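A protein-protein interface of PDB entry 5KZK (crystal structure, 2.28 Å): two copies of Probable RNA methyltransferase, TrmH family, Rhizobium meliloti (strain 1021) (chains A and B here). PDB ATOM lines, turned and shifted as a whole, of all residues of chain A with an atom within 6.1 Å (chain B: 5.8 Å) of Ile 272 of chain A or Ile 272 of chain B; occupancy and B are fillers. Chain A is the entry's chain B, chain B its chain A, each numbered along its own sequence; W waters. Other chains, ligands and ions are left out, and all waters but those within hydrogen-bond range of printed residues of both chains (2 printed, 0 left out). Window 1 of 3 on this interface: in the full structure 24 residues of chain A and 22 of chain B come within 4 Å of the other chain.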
ATOM      1  N   TYR A 220      30.455 -28.231  26.404  1.00  0.00           N
ATOM      2  CA  TYR A 220      30.071 -28.364  24.972  1.00  0.00           C
ATOM      3  C   TYR A 220      31.174 -27.986  23.959  1.00  0.00           C
ATOM      4  O   TYR A 220      31.228 -28.508  22.771  1.00  0.00           O
ATOM      5  CB  TYR A 220      28.773 -27.542  24.724  1.00  0.00           C
ATOM      6  CG  TYR A 220      28.941 -26.006  24.549  1.00  0.00           C
ATOM      7  CD1 TYR A 220      29.271 -25.194  25.592  1.00  0.00           C
ATOM      8  CD2 TYR A 220      28.694 -25.383  23.334  1.00  0.00           C
ATOM      9  CE1 TYR A 220      29.429 -23.816  25.433  1.00  0.00           C
ATOM     10  CE2 TYR A 220      28.818 -23.993  23.160  1.00  0.00           C
ATOM     11  CZ  TYR A 220      29.189 -23.212  24.189  1.00  0.00           C
ATOM     12  OH  TYR A 220      29.324 -21.810  24.097  1.00  0.00           O
ATOM     13  N   ILE A 255      26.470 -26.317  28.725  1.00  0.00           N
ATOM     14  CA  ILE A 255      26.889 -24.947  28.476  1.00  0.00           C
ATOM     15  C   ILE A 255      27.198 -24.202  29.764  1.00  0.00           C
ATOM     16  O   ILE A 255      26.283 -23.939  30.551  1.00  0.00           O
ATOM     17  CB  ILE A 255      25.813 -24.160  27.681  1.00  0.00           C
ATOM     18  CG1 ILE A 255      25.643 -24.773  26.278  1.00  0.00           C
ATOM     19  CG2 ILE A 255      26.295 -22.701  27.528  1.00  0.00           C
ATOM     20  CD1 ILE A 255      24.268 -24.562  25.759  1.00  0.00           C
ATOM     21  N   LEU A 264      19.046 -22.066  30.471  1.00  0.00           N
ATOM     22  CA  LEU A 264      18.822 -21.417  29.159  1.00  0.00           C
ATOM     23  C   LEU A 264      17.479 -21.831  28.601  1.00  0.00           C
ATOM     24  O   LEU A 264      17.101 -22.972  28.727  1.00  0.00           O
ATOM     25  CB  LEU A 264      19.932 -21.839  28.200  1.00  0.00           C
ATOM     26  CG  LEU A 264      21.269 -21.193  28.565  1.00  0.00           C
ATOM     27  CD1 LEU A 264      22.256 -21.733  27.594  1.00  0.00           C
ATOM     28  CD2 LEU A 264      21.287 -19.686  28.543  1.00  0.00           C
ATOM     29  N   ALA A 267      15.361 -23.232  23.032  1.00  0.00           N
ATOM     30  CA  ALA A 267      15.712 -22.762  21.750  1.00  0.00           C
ATOM     31  C   ALA A 267      17.048 -21.977  21.772  1.00  0.00           C
ATOM     32  O   ALA A 267      17.840 -22.122  20.866  1.00  0.00           O
ATOM     33  CB  ALA A 267      14.631 -21.919  21.218  1.00  0.00           C
ATOM     34  N   ILE A 268      17.338 -21.186  22.836  1.00  0.00           N
ATOM     35  CA  ILE A 268      18.654 -20.455  22.862  1.00  0.00           C
ATOM     36  C   ILE A 268      19.729 -21.474  22.966  1.00  0.00           C
ATOM     37  O   ILE A 268      20.790 -21.417  22.323  1.00  0.00           O
ATOM     38  CB  ILE A 268      18.673 -19.469  24.042  1.00  0.00           C
ATOM     39  CG1 ILE A 268      17.605 -18.398  23.854  1.00  0.00           C
ATOM     40  CG2 ILE A 268      20.049 -18.962  24.460  1.00  0.00           C
ATOM     41  CD1 ILE A 268      18.057 -17.378  22.880  1.00  0.00           C
ATOM     42  N   ALA A 269      19.477 -22.462  23.824  1.00  0.00           N
ATOM     43  CA  ALA A 269      20.496 -23.490  24.081  1.00  0.00           C
ATOM     44  C   ALA A 269      20.739 -24.307  22.845  1.00  0.00           C
ATOM     45  O   ALA A 269      21.919 -24.610  22.509  1.00  0.00           O
ATOM     46  CB  ALA A 269      20.059 -24.382  25.202  1.00  0.00           C
ATOM     47  N   THR A 270      19.652 -24.619  22.111  1.00  0.00           N
ATOM     48  CA  THR A 270      19.806 -25.329  20.864  1.00  0.00           C
ATOM     49  C   THR A 270      20.565 -24.496  19.866  1.00  0.00           C
ATOM     50  O   THR A 270      21.388 -25.030  19.136  1.00  0.00           O
ATOM     51  CB  THR A 270      18.461 -25.766  20.287  1.00  0.00           C
ATOM     52  OG1 THR A 270      17.735 -26.552  21.221  1.00  0.00           O
ATOM     53  CG2 THR A 270      18.612 -26.602  19.140  1.00  0.00           C
ATOM     54  N   GLY A 271      20.328 -23.191  19.776  1.00  0.00           N
ATOM     55  CA  GLY A 271      21.067 -22.356  18.821  1.00  0.00           C
ATOM     56  C   GLY A 271      22.572 -22.344  19.114  1.00  0.00           C
ATOM     57  O   GLY A 271      23.451 -22.472  18.197  1.00  0.00           O
ATOM     58  N   ILE A 272      22.875 -22.230  20.408  1.00  0.00           N
ATOM     59  CA  ILE A 272      24.260 -22.248  20.830  1.00  0.00           C
ATOM     60  C   ILE A 272      24.903 -23.581  20.511  1.00  0.00           C
ATOM     61  O   ILE A 272      25.927 -23.624  19.945  1.00  0.00           O
ATOM     62  CB  ILE A 272      24.361 -22.016  22.337  1.00  0.00           C
ATOM     63  CG1 ILE A 272      24.005 -20.579  22.618  1.00  0.00           C
ATOM     64  CG2 ILE A 272      25.795 -22.305  22.759  1.00  0.00           C
ATOM     65  CD1 ILE A 272      23.852 -20.290  24.095  1.00  0.00           C
ATOM     66  N   MET A 273      24.231 -24.690  20.789  1.00  0.00           N
ATOM     67  CA  MET A 273      24.731 -25.998  20.324  1.00  0.00           C
ATOM     68  C   MET A 273      24.909 -26.070  18.850  1.00  0.00           C
ATOM     69  O   MET A 273      25.896 -26.658  18.358  1.00  0.00           O
ATOM     70  CB  MET A 273      23.867 -27.184  20.767  1.00  0.00           C
ATOM     71  CG  MET A 273      23.756 -27.391  22.263  1.00  0.00           C
ATOM     72  SD  MET A 273      25.513 -27.596  23.203  1.00  0.00           S
ATOM     73  CE  MET A 273      26.019 -29.140  22.158  1.00  0.00           C
ATOM     74  N   LEU A 274      23.955 -25.599  18.088  1.00  0.00           N
ATOM     75  CA  LEU A 274      24.083 -25.790  16.653  1.00  0.00           C
ATOM     76  C   LEU A 274      25.305 -25.009  16.121  1.00  0.00           C
ATOM     77  O   LEU A 274      26.090 -25.487  15.319  1.00  0.00           O
ATOM     78  CB  LEU A 274      22.888 -25.255  15.927  1.00  0.00           C
ATOM     79  CG  LEU A 274      21.822 -26.198  15.673  1.00  0.00           C
ATOM     80  CD1 LEU A 274      20.542 -25.526  15.369  1.00  0.00           C
ATOM     81  CD2 LEU A 274      22.166 -27.108  14.556  1.00  0.00           C
ATOM     82  N   PHE A 275      25.468 -23.821  16.591  1.00  0.00           N
ATOM     83  CA  PHE A 275      26.578 -23.002  16.098  1.00  0.00           C
ATOM     84  C   PHE A 275      27.919 -23.398  16.644  1.00  0.00           C
ATOM     85  O   PHE A 275      28.869 -22.884  16.143  1.00  0.00           O
ATOM     86  CB  PHE A 275      26.276 -21.498  16.304  1.00  0.00           C
ATOM     87  CG  PHE A 275      25.375 -20.997  15.213  1.00  0.00           C
ATOM     88  CD1 PHE A 275      23.978 -21.113  15.298  1.00  0.00           C
ATOM     89  CD2 PHE A 275      25.944 -20.458  14.052  1.00  0.00           C
ATOM     90  CE1 PHE A 275      23.200 -20.732  14.283  1.00  0.00           C
ATOM     91  CE2 PHE A 275      25.155 -20.044  13.010  1.00  0.00           C
ATOM     92  CZ  PHE A 275      23.782 -20.168  13.112  1.00  0.00           C
ATOM     93  N   GLU A 276      28.018 -24.314  17.641  1.00  0.00           N
ATOM     94  CA  GLU A 276      29.300 -24.885  18.009  1.00  0.00           C
ATOM     95  C   GLU A 276      29.585 -26.187  17.260  1.00  0.00           C
ATOM     96  O   GLU A 276      30.685 -26.434  16.838  1.00  0.00           O
ATOM     97  CB  GLU A 276      29.294 -25.173  19.517  1.00  0.00           C
ATOM     98  CG  GLU A 276      30.670 -25.570  20.072  1.00  0.00           C
ATOM     99  CD  GLU A 276      31.595 -24.359  20.220  1.00  0.00           C
ATOM    100  OE1 GLU A 276      31.111 -23.171  20.235  1.00  0.00           O
ATOM    101  OE2 GLU A 276      32.827 -24.598  20.307  1.00  0.00           O
ATOM    102  N   ALA A 277      28.578 -27.051  17.140  1.00  0.00           N
ATOM    103  CA  ALA A 277      28.713 -28.237  16.296  1.00  0.00           C
ATOM    104  C   ALA A 277      29.084 -27.898  14.906  1.00  0.00           C
ATOM    105  O   ALA A 277      29.549 -28.754  14.157  1.00  0.00           O
ATOM    106  CB  ALA A 277      27.428 -28.975  16.226  1.00  0.00           C
ATOM    107  N   TYR B 220      31.758 -12.947  13.359  1.00  0.00           N
ATOM    108  CA  TYR B 220      31.686 -12.711  14.817  1.00  0.00           C
ATOM    109  C   TYR B 220      32.748 -13.374  15.663  1.00  0.00           C
ATOM    110  O   TYR B 220      33.030 -12.899  16.723  1.00  0.00           O
ATOM    111  CB  TYR B 220      30.324 -13.037  15.383  1.00  0.00           C
ATOM    112  CG  TYR B 220      30.041 -14.478  15.563  1.00  0.00           C
ATOM    113  CD1 TYR B 220      29.858 -15.320  14.435  1.00  0.00           C
ATOM    114  CD2 TYR B 220      29.854 -15.021  16.857  1.00  0.00           C
ATOM    115  CE1 TYR B 220      29.581 -16.679  14.555  1.00  0.00           C
ATOM    116  CE2 TYR B 220      29.504 -16.407  17.007  1.00  0.00           C
ATOM    117  CZ  TYR B 220      29.379 -17.227  15.853  1.00  0.00           C
ATOM    118  OH  TYR B 220      29.143 -18.575  15.948  1.00  0.00           O
ATOM    119  N   ILE B 255      26.981 -13.254  12.014  1.00  0.00           N
ATOM    120  CA  ILE B 255      27.042 -14.704  12.207  1.00  0.00           C
ATOM    121  C   ILE B 255      26.841 -15.451  10.871  1.00  0.00           C
ATOM    122  O   ILE B 255      25.774 -15.355  10.296  1.00  0.00           O
ATOM    123  CB  ILE B 255      25.993 -15.133  13.247  1.00  0.00           C
ATOM    124  CG1 ILE B 255      26.295 -14.496  14.589  1.00  0.00           C
ATOM    125  CG2 ILE B 255      25.946 -16.662  13.401  1.00  0.00           C
ATOM    126  CD1 ILE B 255      25.004 -14.204  15.323  1.00  0.00           C
ATOM    127  N   LEU B 264      18.151 -15.057  11.595  1.00  0.00           N
ATOM    128  CA  LEU B 264      18.159 -15.441  12.990  1.00  0.00           C
ATOM    129  C   LEU B 264      17.208 -14.551  13.814  1.00  0.00           C
ATOM    130  O   LEU B 264      17.237 -13.342  13.681  1.00  0.00           O
ATOM    131  CB  LEU B 264      19.547 -15.367  13.561  1.00  0.00           C
ATOM    132  CG  LEU B 264      20.456 -16.414  13.042  1.00  0.00           C
ATOM    133  CD1 LEU B 264      21.769 -16.192  13.760  1.00  0.00           C
ATOM    134  CD2 LEU B 264      19.985 -17.815  13.332  1.00  0.00           C
ATOM    135  N   ALA B 267      16.567 -12.896  19.616  1.00  0.00           N
ATOM    136  CA  ALA B 267      16.975 -13.616  20.862  1.00  0.00           C
ATOM    137  C   ALA B 267      18.041 -14.652  20.634  1.00  0.00           C
ATOM    138  O   ALA B 267      19.057 -14.680  21.342  1.00  0.00           O
ATOM    139  CB  ALA B 267      15.801 -14.197  21.607  1.00  0.00           C
ATOM    140  N   ILE B 268      17.885 -15.441  19.575  1.00  0.00           N
ATOM    141  CA  ILE B 268      18.843 -16.433  19.246  1.00  0.00           C
ATOM    142  C   ILE B 268      20.187 -15.774  18.868  1.00  0.00           C
ATOM    143  O   ILE B 268      21.197 -16.218  19.309  1.00  0.00           O
ATOM    144  CB  ILE B 268      18.322 -17.269  18.073  1.00  0.00           C
ATOM    145  CG1 ILE B 268      17.008 -18.066  18.432  1.00  0.00           C
ATOM    146  CG2 ILE B 268      19.398 -18.125  17.528  1.00  0.00           C
ATOM    147  CD1 ILE B 268      17.242 -19.196  19.349  1.00  0.00           C
ATOM    148  N   ALA B 269      20.202 -14.745  18.028  1.00  0.00           N
ATOM    149  CA  ALA B 269      21.423 -14.105  17.591  1.00  0.00           C
ATOM    150  C   ALA B 269      22.030 -13.458  18.803  1.00  0.00           C
ATOM    151  O   ALA B 269      23.158 -13.469  18.962  1.00  0.00           O
ATOM    152  CB  ALA B 269      21.157 -13.015  16.536  1.00  0.00           C
ATOM    153  N   THR B 270      21.236 -12.914  19.651  1.00  0.00           N
ATOM    154  CA  THR B 270      21.773 -12.259  20.819  1.00  0.00           C
ATOM    155  C   THR B 270      22.461 -13.223  21.779  1.00  0.00           C
ATOM    156  O   THR B 270      23.583 -12.902  22.248  1.00  0.00           O
ATOM    157  CB  THR B 270      20.698 -11.428  21.524  1.00  0.00           C
ATOM    158  OG1 THR B 270      20.454 -10.313  20.690  1.00  0.00           O
ATOM    159  CG2 THR B 270      21.217 -10.871  22.813  1.00  0.00           C
ATOM    160  N   GLY B 271      21.846 -14.392  21.980  1.00  0.00           N
ATOM    161  CA  GLY B 271      22.456 -15.481  22.697  1.00  0.00           C
ATOM    162  C   GLY B 271      23.783 -15.992  22.158  1.00  0.00           C
ATOM    163  O   GLY B 271      24.795 -16.216  22.953  1.00  0.00           O
ATOM    164  N   ILE B 272      23.816 -16.149  20.818  1.00  0.00           N
ATOM    165  CA  ILE B 272      25.033 -16.554  20.152  1.00  0.00           C
ATOM    166  C   ILE B 272      26.164 -15.565  20.413  1.00  0.00           C
ATOM    167  O   ILE B 272      27.280 -15.966  20.718  1.00  0.00           O
ATOM    168  CB  ILE B 272      24.808 -16.762  18.647  1.00  0.00           C
ATOM    169  CG1 ILE B 272      23.768 -17.914  18.386  1.00  0.00           C
ATOM    170  CG2 ILE B 272      26.120 -17.056  17.943  1.00  0.00           C
ATOM    171  CD1 ILE B 272      24.146 -19.121  19.204  1.00  0.00           C
ATOM    172  N   MET B 273      25.878 -14.285  20.254  1.00  0.00           N
ATOM    173  CA  MET B 273      26.840 -13.188  20.496  1.00  0.00           C
ATOM    174  C   MET B 273      27.291 -13.141  21.977  1.00  0.00           C
ATOM    175  O   MET B 273      28.461 -13.006  22.247  1.00  0.00           O
ATOM    176  CB  MET B 273      26.249 -11.831  20.085  1.00  0.00           C
ATOM    177  CG  MET B 273      25.913 -11.546  18.540  1.00  0.00           C
ATOM    178  SD  MET B 273      27.475 -11.896  17.458  1.00  0.00           S
ATOM    179  CE  MET B 273      28.779 -10.684  18.276  1.00  0.00           C
ATOM    180  N   LEU B 274      26.376 -13.252  22.942  1.00  0.00           N
ATOM    181  CA  LEU B 274      26.778 -13.252  24.326  1.00  0.00           C
ATOM    182  C   LEU B 274      27.733 -14.370  24.609  1.00  0.00           C
ATOM    183  O   LEU B 274      28.713 -14.156  25.278  1.00  0.00           O
ATOM    184  CB  LEU B 274      25.630 -13.407  25.272  1.00  0.00           C
ATOM    185  CG  LEU B 274      24.784 -12.225  25.617  1.00  0.00           C
ATOM    186  CD1 LEU B 274      23.356 -12.597  25.981  1.00  0.00           C
ATOM    187  CD2 LEU B 274      25.444 -11.394  26.659  1.00  0.00           C
ATOM    188  N   PHE B 275      27.430 -15.560  24.134  1.00  0.00           N
ATOM    189  CA  PHE B 275      28.281 -16.743  24.369  1.00  0.00           C
ATOM    190  C   PHE B 275      29.655 -16.733  23.632  1.00  0.00           C
ATOM    191  O   PHE B 275      30.583 -17.431  23.979  1.00  0.00           O
ATOM    192  CB  PHE B 275      27.507 -18.080  24.307  1.00  0.00           C
ATOM    193  CG  PHE B 275      26.642 -18.310  25.573  1.00  0.00           C
ATOM    194  CD1 PHE B 275      25.349 -17.775  25.703  1.00  0.00           C
ATOM    195  CD2 PHE B 275      27.135 -19.011  26.650  1.00  0.00           C
ATOM    196  CE1 PHE B 275      24.663 -17.840  26.916  1.00  0.00           C
ATOM    197  CE2 PHE B 275      26.436 -19.124  27.806  1.00  0.00           C
ATOM    198  CZ  PHE B 275      25.198 -18.517  27.981  1.00  0.00           C
ATOM    199  N   GLU B 276      29.777 -15.988  22.573  1.00  0.00           N
ATOM    200  CA  GLU B 276      31.036 -15.768  21.944  1.00  0.00           C
ATOM    201  C   GLU B 276      31.804 -14.653  22.669  1.00  0.00           C
ATOM    202  O   GLU B 276      33.005 -14.776  22.906  1.00  0.00           O
ATOM    203  CB  GLU B 276      30.826 -15.392  20.508  1.00  0.00           C
ATOM    204  CG  GLU B 276      32.143 -15.478  19.723  1.00  0.00           C
ATOM    205  CD  GLU B 276      32.617 -16.941  19.527  1.00  0.00           C
ATOM    206  OE1 GLU B 276      31.757 -17.849  19.409  1.00  0.00           O
ATOM    207  OE2 GLU B 276      33.865 -17.188  19.360  1.00  0.00           O
ATOM    208  N   ALA B 277      31.124 -13.563  23.014  1.00  0.00           N
ATOM    209  CA  ALA B 277      31.810 -12.445  23.634  1.00  0.00           C
ATOM    210  C   ALA B 277      32.363 -12.796  24.988  1.00  0.00           C
ATOM    211  O   ALA B 277      33.291 -12.093  25.420  1.00  0.00           O
ATOM    212  CB  ALA B 277      30.898 -11.228  23.775  1.00  0.00           C
HETATM  213  O   HOH W   1      30.861 -20.040  25.275  1.00  0.00           O
HETATM  214  O   HOH W   2      29.657 -20.852  14.563  1.00  0.00           O
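Printed residues of chain B within 4 Å of Ile 272 of chain A: Ile 272 and Phe 275. Printed residues of chain A within 4 Å of Ile 272 of chain B: Gly 271 (3.6 Å) and Ile 272 (3.5 Å). Printed residues of chain B within 4 Å of Ile 268 of chain A: Ala 267 (3.3 Å) and Ile 268 (3.8 Å). Printed residues of chain B within 4 Å of Ala 267 of chain A: Ile 268 (3.3 Å). Printed residues of chain B within 4 Å of Ile 255 of chain A: Phe 275. Of the printed residues of chain B, Gly 271 of chain A touches Ile 272 (3.6 Å). Printed residues of chain A within 4 Å of Ile 255 of chain B: Phe 275. Glu 276 of chain B touches none of the printed residues of chain A.
Water W1 lies within hydrogen-bond range of the side-chain hydroxyl of Tyr 220 of chain A (2.6 Å) and the backbone carbonyl oxygen of Phe 275 of chain B (2.9 Å). Water W2 lies within hydrogen-bond range of the backbone carbonyl oxygen (O) of Phe 275 of chain A (2.7 Å) and the side-chain hydroxyl (OH) of Tyr 220 of chain B (2.7 Å).
Ile 255 of chain A touches Phe 275 of chain B. Ile 268 of chain B touches Ala 267 of chain A (CD1 to O, 3.3 Å). Ile 268 of chain A touches Ala 267 of chain B (CD1 to O, 3.3 Å). CD1 of Ile 268 of chain A touches N of Ile 268 of chain B, 3.8 Å away. O of Gly 271 of chain A touches CD1 of Ile 272 of chain B (3.6 Å). Ile 272 of chain B touches Ile 272 of chain A. CD1 of Ile 272 of chain A touches CD1 of Phe 275 of chain B, at 3.3 Å. CG2 of Ile 255 of chain B touches CE2 of Phe 275 of chain A, 3.5 Å away.
Ile 255 of chain A touches Phe 275 of chain B, and with the chains exchanged Phe 275 of chain A touches Ile 255 of chain B. Ala 267 of chain A touches Ile 268 of chain B, and with the chains exchanged Ile 268 of chain A touches Ala 267 of chain B. Gly 271 of chain A touches Ile 272 of chain B, but with the chains exchanged Ile 272 of chain A does not touch Gly 271 of chain B (4.3 Å). Ile 272 of chain A touches Phe 275 of chain B, but with the chains exchanged Phe 275 of chain A does not touch Ile 272 of chain B (4.3 Å). Positions printed for both chains: 220, 255, 264, 267, 268, 269, 270, 271, 272, 273, 274, 275, 276 and 277. Of the 8 pairs that touch across the chains among the printed residues, 6 have their exchanged pair printed and touching as well.
Hydrophobic or aromatic side chains of chain B that line the printed part of chain A: Ile 255, Ile 268, Ile 272 and Phe 275. Printed residues of chain A that touch a printed residue of chain B: Ile 255, Ala 267, Ile 268, Gly 271, Ile 272 and Phe 275. Among the printed residues, 8 pairs touch across the chains.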
